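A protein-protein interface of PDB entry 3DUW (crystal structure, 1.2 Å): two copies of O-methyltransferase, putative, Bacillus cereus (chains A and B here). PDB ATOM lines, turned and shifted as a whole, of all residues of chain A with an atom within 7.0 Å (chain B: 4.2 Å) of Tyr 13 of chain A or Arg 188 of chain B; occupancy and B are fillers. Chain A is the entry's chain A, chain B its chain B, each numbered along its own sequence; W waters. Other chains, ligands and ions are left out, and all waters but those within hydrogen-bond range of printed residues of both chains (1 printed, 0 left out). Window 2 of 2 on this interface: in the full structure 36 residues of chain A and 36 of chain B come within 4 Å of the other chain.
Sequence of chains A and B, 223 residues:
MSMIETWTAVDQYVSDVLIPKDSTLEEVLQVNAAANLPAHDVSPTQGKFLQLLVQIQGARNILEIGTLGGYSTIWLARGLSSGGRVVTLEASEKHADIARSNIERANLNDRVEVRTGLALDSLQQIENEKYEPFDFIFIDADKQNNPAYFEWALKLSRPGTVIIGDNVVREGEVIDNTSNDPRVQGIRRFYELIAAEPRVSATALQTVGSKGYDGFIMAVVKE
The backbone carbonyl oxygen of Val 174 of chain B sits at hydrogen-bond distance from the guanidinium group of Arg 188 of chain B, 2.8 Å away.
O of Ile 175 of chain B lies close to OD1 of Asn 177 of chain B, 3.4 Å away.
Among the printed residues, pairs that only touch across the chains: Ala 9 of chain A with Ile 175 of chain B (3.7 Å), Val 10 of chain A with Ile 175 of chain B (3.8 Å), Tyr 13 of chain A with Val 174 of chain B (3.8 Å), Tyr 13 of chain A with Ile 175 of chain B (3.7 Å), Tyr 13 of chain A with Arg 188 of chain B (3.4 Å), Tyr 13 of chain A with Tyr 191 of chain B (3.7 Å), Val 17 of chain A with Tyr 191 of chain B (3.9 Å) and Leu 18 of chain A with Tyr 191 of chain B (3.7 Å).
Tyr 13 of chain A touches just these residues of chain B: Val 174, Ile 175, Arg 188 and Tyr 191.
Printed residues of chain B within 4 Å of Val 17 of chain A: Tyr 191 (3.9 Å).
Printed residues of chain B within 4 Å of Leu 18 of chain A: Tyr 191 (3.7 Å).
Of chain A, only Tyr 13 comes within 4 Å of Arg 188 of chain B.
The nearest residue of chain A that does not touch Arg 188 of chain B is Val 17 of chain A (6.5 Å).
Hydrophobic or aromatic side chains of chain A that line the printed part of chain B: Ala 9, Val 10, Tyr 13, Val 17 and Leu 18.
Of the 12 printed residues of chain B, 4 touch a printed residue of chain A.
Among the printed residues, no Asp or Glu carboxylate lies within 4 Å of a Lys or Arg side-chain nitrogen of the other chain.
No position is printed for both chains.
Water W1 lies within hydrogen-bond range of the side-chain carboxylate (OE2) of Glu 192 of chain B, the side-chain hydroxyl (OH) of Tyr 13 of chain A and the guanidinium group (NH2) of Arg 188 of chain B.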
ATOM      1  N   TRP A   7       6.237  17.064  21.525  1.00  0.00           N
ATOM      2  CA  TRP A   7       6.405  18.029  22.610  1.00  0.00           C
ATOM      3  C   TRP A   7       6.266  19.454  22.088  1.00  0.00           C
ATOM      4  O   TRP A   7       5.679  20.316  22.747  1.00  0.00           O
ATOM      5  CB  TRP A   7       7.777  17.877  23.273  1.00  0.00           C
ATOM      6  CG  TRP A   7       8.080  16.501  23.777  1.00  0.00           C
ATOM      7  CD1 TRP A   7       7.184  15.556  24.176  1.00  0.00           C
ATOM      8  CD2 TRP A   7       9.381  15.939  23.995  1.00  0.00           C
ATOM      9  NE1 TRP A   7       7.842  14.438  24.631  1.00  0.00           N
ATOM     10  CE2 TRP A   7       9.193  14.648  24.532  1.00  0.00           C
ATOM     11  CE3 TRP A   7      10.687  16.404  23.791  1.00  0.00           C
ATOM     12  CZ2 TRP A   7      10.264  13.813  24.868  1.00  0.00           C
ATOM     13  CZ3 TRP A   7      11.753  15.571  24.126  1.00  0.00           C
ATOM     14  CH2 TRP A   7      11.531  14.292  24.659  1.00  0.00           C
ATOM     15  N   THR A   8       6.816  19.702  20.905  1.00  0.00           N
ATOM     16  CA  THR A   8       6.747  21.025  20.306  1.00  0.00           C
ATOM     17  C   THR A   8       5.308  21.381  19.928  1.00  0.00           C
ATOM     18  O   THR A   8       4.858  22.502  20.166  1.00  0.00           O
ATOM     19  CB  THR A   8       7.663  21.103  19.067  1.00  0.00           C
ATOM     20  OG1 THR A   8       9.020  20.869  19.471  1.00  0.00           O
ATOM     21  CG2 THR A   8       7.570  22.469  18.407  1.00  0.00           C
ATOM     22  N   ALA A   9       4.590  20.420  19.352  1.00  0.00           N
ATOM     23  CA  ALA A   9       3.204  20.639  18.954  1.00  0.00           C
ATOM     24  C   ALA A   9       2.317  20.906  20.166  1.00  0.00           C
ATOM     25  O   ALA A   9       1.424  21.748  20.114  1.00  0.00           O
ATOM     26  CB  ALA A   9       2.686  19.433  18.182  1.00  0.00           C
ATOM     27  N   VAL A  10       2.561  20.185  21.256  1.00  0.00           N
ATOM     28  CA  VAL A  10       1.768  20.388  22.460  1.00  0.00           C
ATOM     29  C   VAL A  10       2.051  21.776  23.032  1.00  0.00           C
ATOM     30  O   VAL A  10       1.128  22.475  23.443  1.00  0.00           O
ATOM     31  CB  VAL A  10       2.061  19.297  23.515  1.00  0.00           C
ATOM     32  CG1 VAL A  10       1.345  19.627  24.821  1.00  0.00           C
ATOM     33  CG2 VAL A  10       1.592  17.944  22.995  1.00  0.00           C
ATOM     34  N   ASP A  11       3.319  22.188  23.043  1.00  0.00           N
ATOM     35  CA  ASP A  11       3.664  23.511  23.553  1.00  0.00           C
ATOM     36  C   ASP A  11       3.031  24.595  22.683  1.00  0.00           C
ATOM     37  O   ASP A  11       2.612  25.636  23.186  1.00  0.00           O
ATOM     38  CB  ASP A  11       5.187  23.687  23.604  1.00  0.00           C
ATOM     39  CG  ASP A  11       5.740  23.586  25.019  1.00  0.00           C
ATOM     40  OD1 ASP A  11       5.006  23.139  25.929  1.00  0.00           O
ATOM     41  OD2 ASP A  11       6.917  23.956  25.216  1.00  0.00           O
ATOM     42  N   GLN A  12       2.952  24.345  21.379  1.00  0.00           N
ATOM     43  CA  GLN A  12       2.349  25.310  20.464  1.00  0.00           C
ATOM     44  C   GLN A  12       0.866  25.456  20.801  1.00  0.00           C
ATOM     45  O   GLN A  12       0.320  26.556  20.777  1.00  0.00           O
ATOM     46  CB  GLN A  12       2.503  24.852  19.008  1.00  0.00           C
ATOM     47  CG  GLN A  12       2.021  25.873  17.980  1.00  0.00           C
ATOM     48  CD  GLN A  12       2.846  27.145  17.994  1.00  0.00           C
ATOM     49  OE1 GLN A  12       4.067  27.110  17.829  1.00  0.00           O
ATOM     50  NE2 GLN A  12       2.183  28.279  18.190  1.00  0.00           N
ATOM     51  N   TYR A  13       0.220  24.337  21.109  1.00  0.00           N
ATOM     52  CA  TYR A  13      -1.190  24.347  21.480  1.00  0.00           C
ATOM     53  C   TYR A  13      -1.378  25.142  22.773  1.00  0.00           C
ATOM     54  O   TYR A  13      -2.221  26.038  22.855  1.00  0.00           O
ATOM     55  CB  TYR A  13      -1.693  22.916  21.688  1.00  0.00           C
ATOM     56  CG  TYR A  13      -3.083  22.847  22.283  1.00  0.00           C
ATOM     57  CD1 TYR A  13      -4.211  23.077  21.498  1.00  0.00           C
ATOM     58  CD2 TYR A  13      -3.268  22.592  23.645  1.00  0.00           C
ATOM     59  CE1 TYR A  13      -5.489  23.057  22.053  1.00  0.00           C
ATOM     60  CE2 TYR A  13      -4.547  22.572  24.209  1.00  0.00           C
ATOM     61  CZ  TYR A  13      -5.649  22.805  23.405  1.00  0.00           C
ATOM     62  OH  TYR A  13      -6.914  22.788  23.950  1.00  0.00           O
ATOM     63  N   VAL A  14      -0.590  24.801  23.790  1.00  0.00           N
ATOM     64  CA  VAL A  14      -0.676  25.474  25.082  1.00  0.00           C
ATOM     65  C   VAL A  14      -0.480  26.978  24.942  1.00  0.00           C
ATOM     66  O   VAL A  14      -1.250  27.764  25.488  1.00  0.00           O
ATOM     67  CB  VAL A  14       0.375  24.911  26.073  1.00  0.00           C
ATOM     68  CG1 VAL A  14       0.383  25.731  27.358  1.00  0.00           C
ATOM     69  CG2 VAL A  14       0.063  23.455  26.381  1.00  0.00           C
ATOM     70  N   SER A  15       0.550  27.374  24.202  1.00  0.00           N
ATOM     71  CA  SER A  15       0.831  28.790  24.003  1.00  0.00           C
ATOM     72  C   SER A  15      -0.289  29.473  23.222  1.00  0.00           C
ATOM     73  O   SER A  15      -0.744  30.554  23.595  1.00  0.00           O
ATOM     74  CB  SER A  15       2.161  28.965  23.265  1.00  0.00           C
ATOM     75  OG  SER A  15       2.508  30.335  23.161  1.00  0.00           O
ATOM     76  N   ASP A  16      -0.742  28.839  22.142  1.00  0.00           N
ATOM     77  CA  ASP A  16      -1.806  29.414  21.327  1.00  0.00           C
ATOM     78  C   ASP A  16      -3.058  29.713  22.133  1.00  0.00           C
ATOM     79  O   ASP A  16      -3.666  30.772  21.984  1.00  0.00           O
ATOM     80  CB  ASP A  16      -2.188  28.478  20.177  1.00  0.00           C
ATOM     81  CG  ASP A  16      -1.180  28.484  19.053  1.00  0.00           C
ATOM     82  OD1 ASP A  16      -0.354  29.419  18.996  1.00  0.00           O
ATOM     83  OD2 ASP A  16      -1.225  27.554  18.220  1.00  0.00           O
ATOM     84  N   VAL A  17      -3.451  28.780  22.992  1.00  0.00           N
ATOM     85  CA  VAL A  17      -4.659  28.969  23.772  1.00  0.00           C
ATOM     86  C   VAL A  17      -4.510  29.797  25.046  1.00  0.00           C
ATOM     87  O   VAL A  17      -5.358  30.636  25.333  1.00  0.00           O
ATOM     88  CB  VAL A  17      -5.296  27.605  24.143  1.00  0.00           C
ATOM     89  CG1 VAL A  17      -5.601  26.817  22.882  1.00  0.00           C
ATOM     90  CG2 VAL A  17      -4.366  26.815  25.046  1.00  0.00           C
ATOM     91  N   LEU A  18      -3.431  29.583  25.791  1.00  0.00           N
ATOM     92  CA  LEU A  18      -3.241  30.277  27.066  1.00  0.00           C
ATOM     93  C   LEU A  18      -2.403  31.544  27.080  1.00  0.00           C
ATOM     94  O   LEU A  18      -2.436  32.287  28.064  1.00  0.00           O
ATOM     95  CB  LEU A  18      -2.652  29.309  28.097  1.00  0.00           C
ATOM     96  CG  LEU A  18      -3.425  28.019  28.386  1.00  0.00           C
ATOM     97  CD1 LEU A  18      -2.705  27.233  29.470  1.00  0.00           C
ATOM     98  CD2 LEU A  18      -4.843  28.344  28.828  1.00  0.00           C
ATOM     99  N   ILE A  19      -1.652  31.799  26.016  1.00  0.00           N
ATOM    100  CA  ILE A  19      -0.800  32.982  25.987  1.00  0.00           C
ATOM    101  C   ILE A  19      -1.123  33.887  24.804  1.00  0.00           C
ATOM    102  O   ILE A  19      -0.732  33.609  23.670  1.00  0.00           O
ATOM    103  CB  ILE A  19       0.693  32.573  25.941  1.00  0.00           C
ATOM    104  CG1 ILE A  19       0.999  31.618  27.101  1.00  0.00           C
ATOM    105  CG2 ILE A  19       1.585  33.810  26.020  1.00  0.00           C
ATOM    106  CD1 ILE A  19       2.427  31.091  27.120  1.00  0.00           C
ATOM    107  N   VAL B 174      -3.801  15.615  24.205  1.00  0.00           N
ATOM    108  CA  VAL B 174      -4.486  16.894  24.308  1.00  0.00           C
ATOM    109  C   VAL B 174      -4.615  17.623  22.963  1.00  0.00           C
ATOM    110  O   VAL B 174      -5.551  18.391  22.769  1.00  0.00           O
ATOM    111  CB  VAL B 174      -3.786  17.811  25.351  1.00  0.00           C
ATOM    112  CG1 VAL B 174      -2.387  18.163  24.885  1.00  0.00           C
ATOM    113  CG2 VAL B 174      -4.611  19.066  25.588  1.00  0.00           C
ATOM    114  N   ILE B 175      -3.696  17.381  22.029  1.00  0.00           N
ATOM    115  CA  ILE B 175      -3.787  18.055  20.732  1.00  0.00           C
ATOM    116  C   ILE B 175      -4.607  17.300  19.684  1.00  0.00           C
ATOM    117  O   ILE B 175      -4.741  17.759  18.547  1.00  0.00           O
ATOM    118  CB  ILE B 175      -2.385  18.377  20.131  1.00  0.00           C
ATOM    119  CG1 ILE B 175      -1.595  17.096  19.866  1.00  0.00           C
ATOM    120  CG2 ILE B 175      -1.622  19.306  21.069  1.00  0.00           C
ATOM    121  CD1 ILE B 175      -0.264  17.344  19.176  1.00  0.00           C
ATOM    122  N   ASN B 177      -7.604  17.026  18.406  1.00  0.00           N
ATOM    123  CA  ASN B 177      -8.901  17.686  18.365  1.00  0.00           C
ATOM    124  C   ASN B 177     -10.051  16.818  17.865  1.00  0.00           C
ATOM    125  O   ASN B 177     -11.208  17.083  18.188  1.00  0.00           O
ATOM    126  CB  ASN B 177      -8.827  18.962  17.521  1.00  0.00           C
ATOM    127  CG  ASN B 177      -8.137  18.744  16.192  1.00  0.00           C
ATOM    128  OD1 ASN B 177      -6.910  18.782  16.103  1.00  0.00           O
ATOM    129  ND2 ASN B 177      -8.921  18.508  15.148  1.00  0.00           N
ATOM    130  N   VAL B 184     -10.225  13.714  26.751  1.00  0.00           N
ATOM    131  CA  VAL B 184      -9.480  14.609  25.875  1.00  0.00           C
ATOM    132  C   VAL B 184     -10.306  15.854  25.559  1.00  0.00           C
ATOM    133  O   VAL B 184      -9.801  16.974  25.624  1.00  0.00           O
ATOM    134  CB  VAL B 184      -9.089  13.905  24.555  1.00  0.00           C
ATOM    135  CG1 VAL B 184      -8.457  14.902  23.595  1.00  0.00           C
ATOM    136  CG2 VAL B 184      -8.111  12.770  24.846  1.00  0.00           C
ATOM    137  N   GLN B 185     -11.577  15.664  25.218  1.00  0.00           N
ATOM    138  CA  GLN B 185     -12.424  16.805  24.904  1.00  0.00           C
ATOM    139  C   GLN B 185     -12.648  17.685  26.132  1.00  0.00           C
ATOM    140  O   GLN B 185     -12.652  18.909  26.020  1.00  0.00           O
ATOM    141  CB  GLN B 185     -13.760  16.337  24.317  1.00  0.00           C
ATOM    142  CG  GLN B 185     -13.599  15.667  22.954  1.00  0.00           C
ATOM    143  CD  GLN B 185     -12.984  16.584  21.904  1.00  0.00           C
ATOM    144  OE1 GLN B 185     -12.455  16.117  20.892  1.00  0.00           O
ATOM    145  NE2 GLN B 185     -13.058  17.889  22.133  1.00  0.00           N
ATOM    146  N   GLY B 186     -12.819  17.069  27.297  1.00  0.00           N
ATOM    147  CA  GLY B 186     -13.020  17.837  28.516  1.00  0.00           C
ATOM    148  C   GLY B 186     -11.786  18.653  28.859  1.00  0.00           C
ATOM    149  O   GLY B 186     -11.880  19.807  29.280  1.00  0.00           O
ATOM    150  N   ILE B 187     -10.615  18.054  28.685  1.00  0.00           N
ATOM    151  CA  ILE B 187      -9.378  18.756  28.975  1.00  0.00           C
ATOM    152  C   ILE B 187      -9.210  19.936  28.016  1.00  0.00           C
ATOM    153  O   ILE B 187      -8.860  21.039  28.433  1.00  0.00           O
ATOM    154  CB  ILE B 187      -8.172  17.794  28.875  1.00  0.00           C
ATOM    155  CG1 ILE B 187      -8.158  16.852  30.086  1.00  0.00           C
ATOM    156  CG2 ILE B 187      -6.886  18.574  28.768  1.00  0.00           C
ATOM    157  CD1 ILE B 187      -7.868  17.535  31.401  1.00  0.00           C
ATOM    158  N   ARG B 188      -9.472  19.719  26.731  1.00  0.00           N
ATOM    159  CA  ARG B 188      -9.342  20.801  25.764  1.00  0.00           C
ATOM    160  C   ARG B 188     -10.304  21.947  26.088  1.00  0.00           C
ATOM    161  O   ARG B 188      -9.932  23.117  26.003  1.00  0.00           O
ATOM    162  CB  ARG B 188      -9.585  20.280  24.346  1.00  0.00           C
ATOM    163  CG  ARG B 188      -8.443  19.417  23.811  1.00  0.00           C
ATOM    164  CD  ARG B 188      -8.799  18.797  22.470  1.00  0.00           C
ATOM    165  NE  ARG B 188      -9.059  19.803  21.444  1.00  0.00           N
ATOM    166  CZ  ARG B 188      -8.118  20.439  20.753  1.00  0.00           C
ATOM    167  NH1 ARG B 188      -6.838  20.172  20.968  1.00  0.00           N
ATOM    168  NH2 ARG B 188      -8.456  21.349  19.847  1.00  0.00           N
ATOM    169  N   ARG B 189     -11.534  21.622  26.471  1.00  0.00           N
ATOM    170  CA  ARG B 189     -12.493  22.671  26.812  1.00  0.00           C
ATOM    171  C   ARG B 189     -12.061  23.425  28.073  1.00  0.00           C
ATOM    172  O   ARG B 189     -12.385  24.596  28.243  1.00  0.00           O
ATOM    173  CB  ARG B 189     -13.896  22.075  26.971  1.00  0.00           C
ATOM    174  CG  ARG B 189     -14.463  21.577  25.649  1.00  0.00           C
ATOM    175  CD  ARG B 189     -15.702  20.724  25.840  1.00  0.00           C
ATOM    176  NE  ARG B 189     -16.023  19.997  24.616  1.00  0.00           N
ATOM    177  CZ  ARG B 189     -16.700  18.855  24.589  1.00  0.00           C
ATOM    178  NH1 ARG B 189     -17.125  18.312  25.722  1.00  0.00           N
ATOM    179  NH2 ARG B 189     -16.948  18.254  23.432  1.00  0.00           N
ATOM    180  N   PHE B 190     -11.325  22.743  28.945  1.00  0.00           N
ATOM    181  CA  PHE B 190     -10.787  23.332  30.173  1.00  0.00           C
ATOM    182  C   PHE B 190      -9.802  24.444  29.745  1.00  0.00           C
ATOM    183  O   PHE B 190      -9.885  25.578  30.220  1.00  0.00           O
ATOM    184  CB  PHE B 190     -10.094  22.213  30.965  1.00  0.00           C
ATOM    185  CG  PHE B 190      -9.476  22.638  32.271  1.00  0.00           C
ATOM    186  CD1 PHE B 190     -10.238  23.200  33.289  1.00  0.00           C
ATOM    187  CD2 PHE B 190      -8.132  22.384  32.511  1.00  0.00           C
ATOM    188  CE1 PHE B 190      -9.658  23.495  34.531  1.00  0.00           C
ATOM    189  CE2 PHE B 190      -7.545  22.673  33.739  1.00  0.00           C
ATOM    190  CZ  PHE B 190      -8.305  23.228  34.751  1.00  0.00           C
ATOM    191  N   TYR B 191      -8.882  24.127  28.834  1.00  0.00           N
ATOM    192  CA  TYR B 191      -7.928  25.126  28.340  1.00  0.00           C
ATOM    193  C   TYR B 191      -8.689  26.306  27.725  1.00  0.00           C
ATOM    194  O   TYR B 191      -8.387  27.470  27.995  1.00  0.00           O
ATOM    195  CB  TYR B 191      -7.023  24.528  27.252  1.00  0.00           C
ATOM    196  CG  TYR B 191      -5.844  23.709  27.734  1.00  0.00           C
ATOM    197  CD1 TYR B 191      -4.599  24.300  27.958  1.00  0.00           C
ATOM    198  CD2 TYR B 191      -5.957  22.331  27.907  1.00  0.00           C
ATOM    199  CE1 TYR B 191      -3.493  23.531  28.338  1.00  0.00           C
ATOM    200  CE2 TYR B 191      -4.864  21.560  28.283  1.00  0.00           C
ATOM    201  CZ  TYR B 191      -3.634  22.160  28.496  1.00  0.00           C
ATOM    202  OH  TYR B 191      -2.546  21.389  28.857  1.00  0.00           O
ATOM    203  N   GLU B 192      -9.669  25.989  26.883  1.00  0.00           N
ATOM    204  CA  GLU B 192     -10.468  27.003  26.200  1.00  0.00           C
ATOM    205  C   GLU B 192     -11.233  27.913  27.151  1.00  0.00           C
ATOM    206  O   GLU B 192     -11.271  29.131  26.959  1.00  0.00           O
ATOM    207  CB  GLU B 192     -11.451  26.334  25.230  1.00  0.00           C
ATOM    208  CG  GLU B 192     -10.791  25.671  24.024  1.00  0.00           C
ATOM    209  CD  GLU B 192     -11.728  24.735  23.277  1.00  0.00           C
ATOM    210  OE1 GLU B 192     -12.959  24.899  23.394  1.00  0.00           O
ATOM    211  OE2 GLU B 192     -11.236  23.836  22.564  1.00  0.00           O
HETATM  212  O   HOH W   1      -8.819  23.616  22.214  1.00  0.00           O
